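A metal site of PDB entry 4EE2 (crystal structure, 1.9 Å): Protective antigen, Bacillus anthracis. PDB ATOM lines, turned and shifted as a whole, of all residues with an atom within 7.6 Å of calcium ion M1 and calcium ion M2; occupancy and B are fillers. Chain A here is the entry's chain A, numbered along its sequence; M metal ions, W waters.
N of Glu 225 sits at hydrogen-bond distance from OG of Ser 223, at 2.9 Å. The side-chain hydroxyl (OG1) of Thr 229 lies within hydrogen-bond range of the backbone NH (N) of Ser 223, 2.8 Å away. The backbone NH (N) of Lys 226 sits at hydrogen-bond distance from the side-chain hydroxyl (OG) of Ser 223 (3.2 Å). O of Glu 189 sits at hydrogen-bond distance from N of Ser 222, 3.0 Å away. The side-chain carboxylate (OD1) of Asp 236 sits at hydrogen-bond distance from the backbone NH (N) of Thr 229 (2.8 Å). N of Asp 236 lies within hydrogen-bond range of O of Trp 227 (3.0 Å). N of Gly 183 lies within hydrogen-bond range of OD2 of Asp 178, at 2.6 Å. The backbone carbonyl oxygen (O) of Pro 224 lies close to the backbone NH (N) of Asp 180, at 3.4 Å.
Five residues have an atom within 4 Å of calcium ion M1: Asp 178, Asp 180, Asp 182, Ile 184 and Glu 189.
Merely in contact with calcium ion M2: Thr 229 (3.997 Å). Of the 26 residues printed, 7 come within 4 Å of calcium ion M2.
Calcium ion M1 is bound by water W1 (2.1 Å), the side-chain carboxylate of Asp 178 (2.2 Å), the backbone carbonyl oxygen of Ile 184 (2.3 Å), the side-chain carboxylate of Asp 180 (2.3 Å), the side-chain carboxylate of Glu 189 (2.3 Å) and the side-chain carboxylate of Asp 182 (2.4 Å).
Calcium ion M2 is bound by the side-chain carboxylate (OD2) of Asp 182 (2.3 Å), the side-chain carboxylate (OD2) of Asp 180 (2.3 Å), the backbone carbonyl oxygen (O) of Ser 223 (2.4 Å), the side-chain carboxylate (OE1) of Glu 189 (2.4 Å), the side-chain carboxylate (OD2) of Asp 236 (2.4 Å), the backbone carbonyl oxygen (O) of Lys 226 (2.4 Å) and the side-chain carboxylate (OE2) of Glu 189 (2.8 Å). Calcium ion M2 has seven donor atoms within binding distance.
Water W1 lies within hydrogen-bond range of OD1 of Asp 186 (2.7 Å) and O of Pro 224 (2.9 Å).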
ATOM      1  N   TYR A  23      22.706  -5.555 -25.891  1.00  0.00           N
ATOM      2  CA  TYR A  23      21.351  -5.821 -25.426  1.00  0.00           C
ATOM      3  C   TYR A  23      20.389  -5.724 -26.604  1.00  0.00           C
ATOM      4  O   TYR A  23      20.266  -4.669 -27.197  1.00  0.00           O
ATOM      5  CB  TYR A  23      20.922  -4.799 -24.368  1.00  0.00           C
ATOM      6  CG  TYR A  23      21.769  -4.832 -23.118  1.00  0.00           C
ATOM      7  CD1 TYR A  23      22.744  -3.875 -22.889  1.00  0.00           C
ATOM      8  CD2 TYR A  23      21.614  -5.846 -22.179  1.00  0.00           C
ATOM      9  CE1 TYR A  23      23.526  -3.904 -21.739  1.00  0.00           C
ATOM     10  CE2 TYR A  23      22.377  -5.884 -21.041  1.00  0.00           C
ATOM     11  CZ  TYR A  23      23.326  -4.912 -20.823  1.00  0.00           C
ATOM     12  OH  TYR A  23      24.080  -4.970 -19.680  1.00  0.00           O
ATOM     13  N   PRO A 177      18.837  -0.951 -17.799  1.00  0.00           N
ATOM     14  CA  PRO A 177      18.500  -1.076 -16.382  1.00  0.00           C
ATOM     15  C   PRO A 177      19.352  -2.157 -15.746  1.00  0.00           C
ATOM     16  O   PRO A 177      19.022  -3.339 -15.808  1.00  0.00           O
ATOM     17  CB  PRO A 177      17.031  -1.494 -16.407  1.00  0.00           C
ATOM     18  CG  PRO A 177      16.512  -0.906 -17.661  1.00  0.00           C
ATOM     19  CD  PRO A 177      17.635  -0.966 -18.659  1.00  0.00           C
ATOM     20  N   ASP A 178      20.442  -1.728 -15.118  1.00  0.00           N
ATOM     21  CA  ASP A 178      21.328  -2.645 -14.420  1.00  0.00           C
ATOM     22  C   ASP A 178      21.707  -2.040 -13.067  1.00  0.00           C
ATOM     23  O   ASP A 178      22.839  -1.588 -12.889  1.00  0.00           O
ATOM     24  CB  ASP A 178      22.578  -2.884 -15.258  1.00  0.00           C
ATOM     25  CG  ASP A 178      23.423  -4.028 -14.731  1.00  0.00           C
ATOM     26  OD1 ASP A 178      22.924  -4.789 -13.872  1.00  0.00           O
ATOM     27  OD2 ASP A 178      24.576  -4.170 -15.182  1.00  0.00           O
ATOM     28  N   ARG A 179      20.763  -2.008 -12.130  1.00  0.00           N
ATOM     29  CA  ARG A 179      21.022  -1.391 -10.827  1.00  0.00           C
ATOM     30  C   ARG A 179      22.349  -1.812 -10.165  1.00  0.00           C
ATOM     31  O   ARG A 179      23.007  -0.992  -9.530  1.00  0.00           O
ATOM     32  CB  ARG A 179      19.816  -1.668  -9.888  1.00  0.00           C
ATOM     33  CG  ARG A 179      18.512  -1.031 -10.370  1.00  0.00           C
ATOM     34  CD  ARG A 179      17.249  -1.551  -9.664  1.00  0.00           C
ATOM     35  NE  ARG A 179      16.984  -0.897  -8.377  1.00  0.00           N
ATOM     36  CZ  ARG A 179      16.446   0.313  -8.249  1.00  0.00           C
ATOM     37  NH1 ARG A 179      16.137   1.023  -9.327  1.00  0.00           N
ATOM     38  NH2 ARG A 179      16.238   0.818  -7.042  1.00  0.00           N
ATOM     39  N   ASP A 180      22.769  -3.072 -10.322  1.00  0.00           N
ATOM     40  CA  ASP A 180      23.980  -3.539  -9.626  1.00  0.00           C
ATOM     41  C   ASP A 180      25.229  -3.582 -10.506  1.00  0.00           C
ATOM     42  O   ASP A 180      26.313  -3.938 -10.045  1.00  0.00           O
ATOM     43  CB  ASP A 180      23.747  -4.897  -8.968  1.00  0.00           C
ATOM     44  CG  ASP A 180      23.232  -5.941  -9.950  1.00  0.00           C
ATOM     45  OD1 ASP A 180      23.311  -5.719 -11.173  1.00  0.00           O
ATOM     46  OD2 ASP A 180      22.765  -6.984  -9.475  1.00  0.00           O
ATOM     47  N   ASN A 181      25.060  -3.214 -11.765  1.00  0.00           N
ATOM     48  CA  ASN A 181      26.169  -3.116 -12.710  1.00  0.00           C
ATOM     49  C   ASN A 181      26.854  -4.461 -12.966  1.00  0.00           C
ATOM     50  O   ASN A 181      28.029  -4.497 -13.307  1.00  0.00           O
ATOM     51  CB  ASN A 181      27.214  -2.069 -12.260  1.00  0.00           C
ATOM     52  CG  ASN A 181      28.149  -1.633 -13.394  1.00  0.00           C
ATOM     53  OD1 ASN A 181      29.334  -1.393 -13.189  1.00  0.00           O
ATOM     54  ND2 ASN A 181      27.612  -1.541 -14.599  1.00  0.00           N
ATOM     55  N   ASP A 182      26.125  -5.566 -12.849  1.00  0.00           N
ATOM     56  CA  ASP A 182      26.748  -6.832 -13.208  1.00  0.00           C
ATOM     57  C   ASP A 182      26.639  -7.147 -14.694  1.00  0.00           C
ATOM     58  O   ASP A 182      27.395  -7.983 -15.207  1.00  0.00           O
ATOM     59  CB  ASP A 182      26.268  -7.994 -12.322  1.00  0.00           C
ATOM     60  CG  ASP A 182      24.764  -8.223 -12.393  1.00  0.00           C
ATOM     61  OD1 ASP A 182      24.105  -7.803 -13.365  1.00  0.00           O
ATOM     62  OD2 ASP A 182      24.261  -8.882 -11.471  1.00  0.00           O
ATOM     63  N   GLY A 183      25.738  -6.456 -15.386  1.00  0.00           N
ATOM     64  CA  GLY A 183      25.563  -6.645 -16.820  1.00  0.00           C
ATOM     65  C   GLY A 183      24.244  -7.282 -17.225  1.00  0.00           C
ATOM     66  O   GLY A 183      23.820  -7.177 -18.377  1.00  0.00           O
ATOM     67  N   ILE A 184      23.584  -7.942 -16.282  1.00  0.00           N
ATOM     68  CA  ILE A 184      22.272  -8.515 -16.545  1.00  0.00           C
ATOM     69  C   ILE A 184      21.220  -7.488 -16.177  1.00  0.00           C
ATOM     70  O   ILE A 184      21.195  -7.016 -15.049  1.00  0.00           O
ATOM     71  CB  ILE A 184      22.026  -9.783 -15.715  1.00  0.00           C
ATOM     72  CG1 ILE A 184      23.266 -10.693 -15.737  1.00  0.00           C
ATOM     73  CG2 ILE A 184      20.793 -10.527 -16.227  1.00  0.00           C
ATOM     74  CD1 ILE A 184      23.147 -11.905 -14.855  1.00  0.00           C
ATOM     75  N   PRO A 185      20.355  -7.134 -17.139  1.00  0.00           N
ATOM     76  CA  PRO A 185      19.233  -6.223 -16.931  1.00  0.00           C
ATOM     77  C   PRO A 185      18.404  -6.591 -15.711  1.00  0.00           C
ATOM     78  O   PRO A 185      18.177  -7.776 -15.482  1.00  0.00           O
ATOM     79  CB  PRO A 185      18.399  -6.419 -18.201  1.00  0.00           C
ATOM     80  CG  PRO A 185      19.410  -6.752 -19.252  1.00  0.00           C
ATOM     81  CD  PRO A 185      20.481  -7.547 -18.555  1.00  0.00           C
ATOM     82  N   ASP A 186      17.939  -5.597 -14.952  1.00  0.00           N
ATOM     83  CA  ASP A 186      17.124  -5.844 -13.747  1.00  0.00           C
ATOM     84  C   ASP A 186      16.011  -6.860 -14.017  1.00  0.00           C
ATOM     85  O   ASP A 186      15.791  -7.780 -13.230  1.00  0.00           O
ATOM     86  CB  ASP A 186      16.446  -4.551 -13.268  1.00  0.00           C
ATOM     87  CG  ASP A 186      17.423  -3.437 -12.962  1.00  0.00           C
ATOM     88  OD1 ASP A 186      18.637  -3.690 -12.784  1.00  0.00           O
ATOM     89  OD2 ASP A 186      16.972  -2.271 -12.877  1.00  0.00           O
ATOM     90  N   SER A 187      15.296  -6.661 -15.122  1.00  0.00           N
ATOM     91  CA  SER A 187      14.087  -7.428 -15.386  1.00  0.00           C
ATOM     92  C   SER A 187      14.373  -8.906 -15.619  1.00  0.00           C
ATOM     93  O   SER A 187      13.591  -9.760 -15.229  1.00  0.00           O
ATOM     94  CB  SER A 187      13.300  -6.831 -16.571  1.00  0.00           C
ATOM     95  OG  SER A 187      14.020  -6.949 -17.785  1.00  0.00           O
ATOM     96  N   GLU A 189      17.064 -10.648 -14.337  1.00  0.00           N
ATOM     97  CA  GLU A 189      17.425 -11.280 -13.060  1.00  0.00           C
ATOM     98  C   GLU A 189      16.192 -11.628 -12.242  1.00  0.00           C
ATOM     99  O   GLU A 189      16.123 -12.672 -11.597  1.00  0.00           O
ATOM    100  CB  GLU A 189      18.356 -10.378 -12.244  1.00  0.00           C
ATOM    101  CG  GLU A 189      19.701 -10.146 -12.893  1.00  0.00           C
ATOM    102  CD  GLU A 189      20.764  -9.686 -11.906  1.00  0.00           C
ATOM    103  OE1 GLU A 189      21.180 -10.510 -11.069  1.00  0.00           O
ATOM    104  OE2 GLU A 189      21.151  -8.504 -11.971  1.00  0.00           O
ATOM    105  N   TYR A 193      16.113 -16.196 -16.237  1.00  0.00           N
ATOM    106  CA  TYR A 193      16.850 -16.229 -17.486  1.00  0.00           C
ATOM    107  C   TYR A 193      17.558 -17.563 -17.677  1.00  0.00           C
ATOM    108  O   TYR A 193      17.751 -18.337 -16.742  1.00  0.00           O
ATOM    109  CB  TYR A 193      17.845 -15.075 -17.553  1.00  0.00           C
ATOM    110  CG  TYR A 193      18.841 -14.984 -16.408  1.00  0.00           C
ATOM    111  CD1 TYR A 193      18.475 -14.402 -15.194  1.00  0.00           C
ATOM    112  CD2 TYR A 193      20.147 -15.444 -16.540  1.00  0.00           C
ATOM    113  CE1 TYR A 193      19.389 -14.300 -14.133  1.00  0.00           C
ATOM    114  CE2 TYR A 193      21.059 -15.341 -15.502  1.00  0.00           C
ATOM    115  CZ  TYR A 193      20.673 -14.768 -14.300  1.00  0.00           C
ATOM    116  OH  TYR A 193      21.567 -14.675 -13.252  1.00  0.00           O
ATOM    117  N   SER A 222      18.304 -14.143 -10.071  1.00  0.00           N
ATOM    118  CA  SER A 222      19.285 -13.522  -9.186  1.00  0.00           C
ATOM    119  C   SER A 222      18.762 -12.176  -8.681  1.00  0.00           C
ATOM    120  O   SER A 222      17.717 -11.712  -9.138  1.00  0.00           O
ATOM    121  CB  SER A 222      20.641 -13.384  -9.899  1.00  0.00           C
ATOM    122  OG  SER A 222      20.498 -13.071 -11.285  1.00  0.00           O
ATOM    123  N   SER A 223      19.456 -11.555  -7.739  1.00  0.00           N
ATOM    124  CA  SER A 223      19.059 -10.209  -7.315  1.00  0.00           C
ATOM    125  C   SER A 223      19.528  -9.163  -8.295  1.00  0.00           C
ATOM    126  O   SER A 223      20.689  -9.124  -8.663  1.00  0.00           O
ATOM    127  CB  SER A 223      19.600  -9.834  -5.940  1.00  0.00           C
ATOM    128  OG  SER A 223      19.327  -8.461  -5.680  1.00  0.00           O
ATOM    129  N   PRO A 224      18.619  -8.275  -8.731  1.00  0.00           N
ATOM    130  CA  PRO A 224      19.046  -7.170  -9.578  1.00  0.00           C
ATOM    131  C   PRO A 224      19.810  -6.093  -8.800  1.00  0.00           C
ATOM    132  O   PRO A 224      20.290  -5.136  -9.384  1.00  0.00           O
ATOM    133  CB  PRO A 224      17.716  -6.614 -10.113  1.00  0.00           C
ATOM    134  CG  PRO A 224      16.722  -6.942  -9.059  1.00  0.00           C
ATOM    135  CD  PRO A 224      17.160  -8.288  -8.520  1.00  0.00           C
ATOM    136  N   GLU A 225      19.915  -6.245  -7.485  1.00  0.00           N
ATOM    137  CA  GLU A 225      20.561  -5.242  -6.644  1.00  0.00           C
ATOM    138  C   GLU A 225      21.828  -5.789  -5.953  1.00  0.00           C
ATOM    139  O   GLU A 225      22.481  -5.104  -5.180  1.00  0.00           O
ATOM    140  CB  GLU A 225      19.555  -4.690  -5.653  1.00  0.00           C
ATOM    141  CG  GLU A 225      18.384  -3.996  -6.371  1.00  0.00           C
ATOM    142  CD  GLU A 225      17.428  -3.249  -5.453  1.00  0.00           C
ATOM    143  OE1 GLU A 225      17.793  -2.993  -4.279  1.00  0.00           O
ATOM    144  OE2 GLU A 225      16.299  -2.933  -5.911  1.00  0.00           O
ATOM    145  N   LYS A 226      22.157  -7.032  -6.253  1.00  0.00           N
ATOM    146  CA  LYS A 226      23.378  -7.648  -5.754  1.00  0.00           C
ATOM    147  C   LYS A 226      24.255  -8.050  -6.928  1.00  0.00           C
ATOM    148  O   LYS A 226      23.893  -8.948  -7.700  1.00  0.00           O
ATOM    149  CB  LYS A 226      23.068  -8.854  -4.860  1.00  0.00           C
ATOM    150  CG  LYS A 226      22.286  -8.477  -3.593  1.00  0.00           C
ATOM    151  CD  LYS A 226      21.949  -9.682  -2.706  1.00  0.00           C
ATOM    152  CE  LYS A 226      23.195 -10.300  -2.060  1.00  0.00           C
ATOM    153  NZ  LYS A 226      23.793  -9.410  -1.043  1.00  0.00           N
ATOM    154  N   TRP A 227      25.394  -7.387  -7.053  1.00  0.00           N
ATOM    155  CA  TRP A 227      26.355  -7.648  -8.127  1.00  0.00           C
ATOM    156  C   TRP A 227      26.730  -9.147  -8.109  1.00  0.00           C
ATOM    157  O   TRP A 227      26.753  -9.808  -9.155  1.00  0.00           O
ATOM    158  CB  TRP A 227      27.554  -6.709  -7.963  1.00  0.00           C
ATOM    159  CG  TRP A 227      28.703  -6.933  -8.903  1.00  0.00           C
ATOM    160  CD1 TRP A 227      28.883  -6.385 -10.147  1.00  0.00           C
ATOM    161  CD2 TRP A 227      29.871  -7.722  -8.648  1.00  0.00           C
ATOM    162  NE1 TRP A 227      30.075  -6.808 -10.680  1.00  0.00           N
ATOM    163  CE2 TRP A 227      30.710  -7.618  -9.780  1.00  0.00           C
ATOM    164  CE3 TRP A 227      30.294  -8.518  -7.572  1.00  0.00           C
ATOM    165  CZ2 TRP A 227      31.951  -8.275  -9.874  1.00  0.00           C
ATOM    166  CZ3 TRP A 227      31.521  -9.175  -7.668  1.00  0.00           C
ATOM    167  CH2 TRP A 227      32.333  -9.057  -8.811  1.00  0.00           C
ATOM    168  N   SER A 228      26.997  -9.664  -6.921  1.00  0.00           N
ATOM    169  CA  SER A 228      27.045 -11.105  -6.691  1.00  0.00           C
ATOM    170  C   SER A 228      25.921 -11.460  -5.741  1.00  0.00           C
ATOM    171  O   SER A 228      25.885 -11.006  -4.598  1.00  0.00           O
ATOM    172  CB  SER A 228      28.388 -11.532  -6.066  1.00  0.00           C
ATOM    173  OG  SER A 228      28.332 -12.882  -5.619  1.00  0.00           O
ATOM    174  N   THR A 229      24.970 -12.266  -6.195  1.00  0.00           N
ATOM    175  CA  THR A 229      23.818 -12.552  -5.370  1.00  0.00           C
ATOM    176  C   THR A 229      24.162 -13.383  -4.139  1.00  0.00           C
ATOM    177  O   THR A 229      23.523 -13.250  -3.095  1.00  0.00           O
ATOM    178  CB  THR A 229      22.667 -13.172  -6.206  1.00  0.00           C
ATOM    179  OG1 THR A 229      22.136 -12.142  -7.059  1.00  0.00           O
ATOM    180  CG2 THR A 229      21.558 -13.656  -5.308  1.00  0.00           C
ATOM    181  N   SER A 235      30.699 -12.025 -10.050  1.00  0.00           N
ATOM    182  CA  SER A 235      29.384 -11.468 -10.357  1.00  0.00           C
ATOM    183  C   SER A 235      28.435 -12.487 -10.978  1.00  0.00           C
ATOM    184  O   SER A 235      28.863 -13.470 -11.567  1.00  0.00           O
ATOM    185  CB  SER A 235      29.512 -10.254 -11.281  1.00  0.00           C
ATOM    186  OG  SER A 235      29.293 -10.615 -12.636  1.00  0.00           O
ATOM    187  N   ASP A 236      27.134 -12.217 -10.858  1.00  0.00           N
ATOM    188  CA  ASP A 236      26.117 -13.107 -11.417  1.00  0.00           C
ATOM    189  C   ASP A 236      26.362 -13.311 -12.918  1.00  0.00           C
ATOM    190  O   ASP A 236      26.175 -14.392 -13.454  1.00  0.00           O
ATOM    191  CB  ASP A 236      24.714 -12.512 -11.187  1.00  0.00           C
ATOM    192  CG  ASP A 236      24.363 -12.354  -9.704  1.00  0.00           C
ATOM    193  OD1 ASP A 236      24.910 -13.098  -8.855  1.00  0.00           O
ATOM    194  OD2 ASP A 236      23.523 -11.497  -9.365  1.00  0.00           O
ATOM    195  N   PHE A 237      26.771 -12.233 -13.588  1.00  0.00           N
ATOM    196  CA  PHE A 237      27.069 -12.264 -15.016  1.00  0.00           C
ATOM    197  C   PHE A 237      28.354 -13.034 -15.321  1.00  0.00           C
ATOM    198  O   PHE A 237      28.413 -13.806 -16.280  1.00  0.00           O
ATOM    199  CB  PHE A 237      27.199 -10.836 -15.526  1.00  0.00           C
ATOM    200  CG  PHE A 237      27.436 -10.710 -17.017  1.00  0.00           C
ATOM    201  CD1 PHE A 237      26.388 -10.799 -17.928  1.00  0.00           C
ATOM    202  CD2 PHE A 237      28.702 -10.436 -17.504  1.00  0.00           C
ATOM    203  CE1 PHE A 237      26.607 -10.658 -19.300  1.00  0.00           C
ATOM    204  CE2 PHE A 237      28.935 -10.295 -18.872  1.00  0.00           C
ATOM    205  CZ  PHE A 237      27.896 -10.408 -19.762  1.00  0.00           C
ATOM    206  N   PRO A 255      24.349 -18.339  -9.892  1.00  0.00           N
ATOM    207  CA  PRO A 255      24.353 -17.090  -9.127  1.00  0.00           C
ATOM    208  C   PRO A 255      23.850 -17.266  -7.686  1.00  0.00           C
ATOM    209  O   PRO A 255      24.149 -16.426  -6.834  1.00  0.00           O
ATOM    210  CB  PRO A 255      23.401 -16.181  -9.923  1.00  0.00           C
ATOM    211  CG  PRO A 255      23.570 -16.658 -11.341  1.00  0.00           C
ATOM    212  CD  PRO A 255      23.781 -18.160 -11.239  1.00  0.00           C
HETATM  213 CA    CA M   1      22.084  -6.603 -12.947  1.00  0.00          CA
HETATM  214 CA    CA M   2      22.744  -9.291  -9.794  1.00  0.00          CA
HETATM  215  O   HOH W   1      20.458  -5.546 -12.271  1.00  0.00           O
